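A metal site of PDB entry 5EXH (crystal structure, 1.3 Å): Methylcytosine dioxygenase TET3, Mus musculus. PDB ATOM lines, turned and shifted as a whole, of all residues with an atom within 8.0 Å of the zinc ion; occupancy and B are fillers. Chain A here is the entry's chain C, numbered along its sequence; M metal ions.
The side-chain sulfur (SG) of Cys 8 sits close to the backbone NH (N) of Thr 10. The side-chain carboxylate (OE1) of Glu 41 lies within salt-bridge range of the side-chain amino group (NZ) of Lys 44 (2.8 Å). The side-chain sulfur (SG) of Cys 14 lies close to the backbone NH (N) of Gly 9. The side-chain sulfur (SG) of Cys 40 sits close to the backbone NH (N) of Val 42 (3.4 Å). The side-chain sulfur (SG) of Cys 11 lies close to the backbone NH (N) of Glu 41 (3.5 Å). The side-chain sulfur of Cys 40 lies close to the backbone NH of Leu 43.
N of Gly 9 touches the zinc ion (3.8 Å). Glu 41 touches the zinc ion.
The zinc ion is bound by SG of Cys 8, SG of Cys 11, SG of Cys 40 and SG of Cys 14.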
ATOM      1  N   LYS A   6       2.918  15.679   0.813  1.00  0.00           N
ATOM      2  CA  LYS A   6       2.474  16.550   1.880  1.00  0.00           C
ATOM      3  C   LYS A   6       1.519  17.585   1.303  1.00  0.00           C
ATOM      4  O   LYS A   6       1.597  17.913   0.117  1.00  0.00           O
ATOM      5  CB  LYS A   6       3.666  17.283   2.508  1.00  0.00           C
ATOM      6  CG  LYS A   6       4.897  16.426   2.750  1.00  0.00           C
ATOM      7  CD  LYS A   6       4.706  15.446   3.881  1.00  0.00           C
ATOM      8  CE  LYS A   6       6.053  15.021   4.489  1.00  0.00           C
ATOM      9  NZ  LYS A   6       6.721  16.127   5.226  1.00  0.00           N
ATOM     10  N   ARG A   7       0.622  18.121   2.127  1.00  0.00           N
ATOM     11  CA  ARG A   7      -0.300  19.152   1.689  1.00  0.00           C
ATOM     12  C   ARG A   7       0.467  20.378   1.191  1.00  0.00           C
ATOM     13  O   ARG A   7       1.576  20.670   1.658  1.00  0.00           O
ATOM     14  CB  ARG A   7      -1.296  19.520   2.795  1.00  0.00           C
ATOM     15  CG  ARG A   7      -0.861  20.645   3.750  1.00  0.00           C
ATOM     16  CD  ARG A   7       0.259  20.232   4.701  1.00  0.00           C
ATOM     17  NE  ARG A   7       0.561  21.304   5.650  1.00  0.00           N
ATOM     18  CZ  ARG A   7       1.280  22.382   5.349  1.00  0.00           C
ATOM     19  NH1 ARG A   7       1.500  23.305   6.275  1.00  0.00           N
ATOM     20  NH2 ARG A   7       1.775  22.535   4.132  1.00  0.00           N
ATOM     21  N   CYS A   8      -0.119  21.103   0.251  1.00  0.00           N
ATOM     22  CA  CYS A   8       0.577  22.235  -0.350  1.00  0.00           C
ATOM     23  C   CYS A   8       0.704  23.423   0.598  1.00  0.00           C
ATOM     24  O   CYS A   8       1.670  24.195   0.514  1.00  0.00           O
ATOM     25  CB  CYS A   8      -0.071  22.635  -1.682  1.00  0.00           C
ATOM     26  SG  CYS A   8      -1.502  23.727  -1.562  1.00  0.00           S
ATOM     27  N   GLY A   9      -0.254  23.556   1.519  1.00  0.00           N
ATOM     28  CA  GLY A   9      -0.217  24.620   2.504  1.00  0.00           C
ATOM     29  C   GLY A   9      -0.756  25.959   2.042  1.00  0.00           C
ATOM     30  O   GLY A   9      -0.960  26.851   2.870  1.00  0.00           O
ATOM     31  N   THR A  10      -1.013  26.100   0.744  1.00  0.00           N
ATOM     32  CA  THR A  10      -1.367  27.412   0.198  1.00  0.00           C
ATOM     33  C   THR A  10      -2.755  27.539  -0.411  1.00  0.00           C
ATOM     34  O   THR A  10      -3.281  28.650  -0.525  1.00  0.00           O
ATOM     35  CB  THR A  10      -0.346  27.908  -0.867  1.00  0.00           C
ATOM     36  OG1 THR A  10      -0.449  27.104  -2.047  1.00  0.00           O
ATOM     37  CG2 THR A  10       1.044  27.820  -0.337  1.00  0.00           C
ATOM     38  N   CYS A  11      -3.355  26.422  -0.826  1.00  0.00           N
ATOM     39  CA  CYS A  11      -4.695  26.459  -1.405  1.00  0.00           C
ATOM     40  C   CYS A  11      -5.723  26.804  -0.332  1.00  0.00           C
ATOM     41  O   CYS A  11      -5.432  26.720   0.862  1.00  0.00           O
ATOM     42  CB  CYS A  11      -5.045  25.124  -2.088  1.00  0.00           C
ATOM     43  SG  CYS A  11      -5.280  23.713  -0.974  1.00  0.00           S
ATOM     44  N   ASP A  12      -6.913  27.193  -0.755  1.00  0.00           N
ATOM     45  CA  ASP A  12      -7.931  27.582   0.223  1.00  0.00           C
ATOM     46  C   ASP A  12      -8.270  26.472   1.240  1.00  0.00           C
ATOM     47  O   ASP A  12      -8.340  26.747   2.441  1.00  0.00           O
ATOM     48  CB  ASP A  12      -9.169  28.187  -0.456  1.00  0.00           C
ATOM     49  CG  ASP A  12      -8.906  29.585  -1.006  1.00  0.00           C
ATOM     50  OD1 ASP A  12      -8.760  30.524  -0.199  1.00  0.00           O
ATOM     51  OD2 ASP A  12      -8.831  29.727  -2.256  1.00  0.00           O
ATOM     52  N   PRO A  13      -8.454  25.224   0.781  1.00  0.00           N
ATOM     53  CA  PRO A  13      -8.662  24.146   1.763  1.00  0.00           C
ATOM     54  C   PRO A  13      -7.509  24.012   2.763  1.00  0.00           C
ATOM     55  O   PRO A  13      -7.758  23.824   3.945  1.00  0.00           O
ATOM     56  CB  PRO A  13      -8.783  22.890   0.878  1.00  0.00           C
ATOM     57  CG  PRO A  13      -9.397  23.413  -0.393  1.00  0.00           C
ATOM     58  CD  PRO A  13      -8.742  24.754  -0.591  1.00  0.00           C
ATOM     59  N   CYS A  14      -6.265  24.120   2.299  1.00  0.00           N
ATOM     60  CA  CYS A  14      -5.111  24.061   3.196  1.00  0.00           C
ATOM     61  C   CYS A  14      -5.071  25.189   4.235  1.00  0.00           C
ATOM     62  O   CYS A  14      -4.440  25.044   5.292  1.00  0.00           O
ATOM     63  CB  CYS A  14      -3.796  24.047   2.401  1.00  0.00           C
ATOM     64  SG  CYS A  14      -3.308  22.421   1.797  1.00  0.00           S
ATOM     65  N   ARG A  15      -5.729  26.304   3.939  1.00  0.00           N
ATOM     66  CA  ARG A  15      -5.716  27.452   4.836  1.00  0.00           C
ATOM     67  C   ARG A  15      -6.849  27.459   5.858  1.00  0.00           C
ATOM     68  O   ARG A  15      -6.838  28.259   6.791  1.00  0.00           O
ATOM     69  CB  ARG A  15      -5.659  28.756   4.030  1.00  0.00           C
ATOM     70  CG  ARG A  15      -4.296  28.946   3.360  1.00  0.00           C
ATOM     71  CD  ARG A  15      -4.234  30.181   2.470  1.00  0.00           C
ATOM     72  NE  ARG A  15      -2.931  30.318   1.836  1.00  0.00           N
ATOM     73  CZ  ARG A  15      -1.905  30.978   2.359  1.00  0.00           C
ATOM     74  NH1 ARG A  15      -0.746  31.035   1.717  1.00  0.00           N
ATOM     75  NH2 ARG A  15      -2.029  31.574   3.536  1.00  0.00           N
ATOM     76  N   ARG A  38     -11.209  20.603   3.772  1.00  0.00           N
ATOM     77  CA  ARG A  38      -9.784  20.817   4.031  1.00  0.00           C
ATOM     78  C   ARG A  38      -8.871  20.077   3.054  1.00  0.00           C
ATOM     79  O   ARG A  38      -7.678  20.367   2.991  1.00  0.00           O
ATOM     80  CB  ARG A  38      -9.422  20.439   5.478  1.00  0.00           C
ATOM     81  CG  ARG A  38     -10.078  21.331   6.534  1.00  0.00           C
ATOM     82  CD  ARG A  38      -9.599  21.001   7.935  1.00  0.00           C
ATOM     83  NE  ARG A  38      -8.139  20.926   7.946  1.00  0.00           N
ATOM     84  CZ  ARG A  38      -7.422  19.955   8.502  1.00  0.00           C
ATOM     85  NH1 ARG A  38      -8.019  18.967   9.166  1.00  0.00           N
ATOM     86  NH2 ARG A  38      -6.101  19.988   8.391  1.00  0.00           N
ATOM     87  N   LYS A  39      -9.403  19.115   2.293  1.00  0.00           N
ATOM     88  CA  LYS A  39      -8.548  18.306   1.429  1.00  0.00           C
ATOM     89  C   LYS A  39      -7.783  19.197   0.440  1.00  0.00           C
ATOM     90  O   LYS A  39      -8.401  19.993  -0.280  1.00  0.00           O
ATOM     91  CB  LYS A  39      -9.381  17.266   0.671  1.00  0.00           C
ATOM     92  CG  LYS A  39      -8.569  16.399  -0.309  1.00  0.00           C
ATOM     93  CD  LYS A  39      -7.619  15.431   0.398  1.00  0.00           C
ATOM     94  CE  LYS A  39      -6.793  14.616  -0.583  1.00  0.00           C
ATOM     95  NZ  LYS A  39      -6.007  13.527   0.073  1.00  0.00           N
ATOM     96  N   CYS A  40      -6.460  19.058   0.417  1.00  0.00           N
ATOM     97  CA  CYS A  40      -5.610  19.881  -0.430  1.00  0.00           C
ATOM     98  C   CYS A  40      -5.939  19.665  -1.906  1.00  0.00           C
ATOM     99  O   CYS A  40      -6.040  18.524  -2.376  1.00  0.00           O
ATOM    100  CB  CYS A  40      -4.156  19.518  -0.163  1.00  0.00           C
ATOM    101  SG  CYS A  40      -3.003  20.390  -1.233  1.00  0.00           S
ATOM    102  N   GLU A  41      -6.101  20.759  -2.642  1.00  0.00           N
ATOM    103  CA  GLU A  41      -6.405  20.675  -4.070  1.00  0.00           C
ATOM    104  C   GLU A  41      -5.314  19.940  -4.842  1.00  0.00           C
ATOM    105  O   GLU A  41      -5.601  19.198  -5.792  1.00  0.00           O
ATOM    106  CB  GLU A  41      -6.627  22.055  -4.685  1.00  0.00           C
ATOM    107  CG  GLU A  41      -7.673  22.938  -3.976  1.00  0.00           C
ATOM    108  CD  GLU A  41      -9.128  22.493  -4.154  1.00  0.00           C
ATOM    109  OE1 GLU A  41      -9.389  21.364  -4.614  1.00  0.00           O
ATOM    110  OE2 GLU A  41     -10.031  23.304  -3.832  1.00  0.00           O
ATOM    111  N   VAL A  42      -4.052  20.155  -4.453  1.00  0.00           N
ATOM    112  CA  VAL A  42      -2.936  19.527  -5.137  1.00  0.00           C
ATOM    113  C   VAL A  42      -2.948  18.006  -4.929  1.00  0.00           C
ATOM    114  O   VAL A  42      -2.638  17.238  -5.844  1.00  0.00           O
ATOM    115  CB  VAL A  42      -1.594  20.132  -4.670  1.00  0.00           C
ATOM    116  CG1 VAL A  42      -0.409  19.400  -5.308  1.00  0.00           C
ATOM    117  CG2 VAL A  42      -1.536  21.626  -4.979  1.00  0.00           C
ATOM    118  N   LEU A  43      -3.342  17.591  -3.728  1.00  0.00           N
ATOM    119  CA  LEU A  43      -3.362  16.189  -3.364  1.00  0.00           C
ATOM    120  C   LEU A  43      -4.532  15.433  -3.990  1.00  0.00           C
ATOM    121  O   LEU A  43      -4.628  14.211  -3.869  1.00  0.00           O
ATOM    122  CB  LEU A  43      -3.389  16.029  -1.837  1.00  0.00           C
ATOM    123  CG  LEU A  43      -2.124  16.490  -1.105  1.00  0.00           C
ATOM    124  CD1 LEU A  43      -2.253  16.183   0.391  1.00  0.00           C
ATOM    125  CD2 LEU A  43      -0.879  15.828  -1.685  1.00  0.00           C
ATOM    126  N   LYS A  44      -5.423  16.162  -4.681  1.00  0.00           N
ATOM    127  CA  LYS A  44      -6.520  15.515  -5.413  1.00  0.00           C
ATOM    128  C   LYS A  44      -6.045  14.922  -6.749  1.00  0.00           C
ATOM    129  O   LYS A  44      -6.761  14.128  -7.363  1.00  0.00           O
ATOM    130  CB  LYS A  44      -7.712  16.466  -5.599  1.00  0.00           C
ATOM    131  CG  LYS A  44      -8.357  16.867  -4.269  1.00  0.00           C
ATOM    132  CD  LYS A  44      -9.477  17.894  -4.424  1.00  0.00           C
ATOM    133  CE  LYS A  44      -9.896  18.412  -3.062  1.00  0.00           C
ATOM    134  NZ  LYS A  44     -10.948  19.471  -3.189  1.00  0.00           N
HETATM  135 ZN    ZN M   1      -3.266  22.609  -0.553  1.00  0.00          ZN
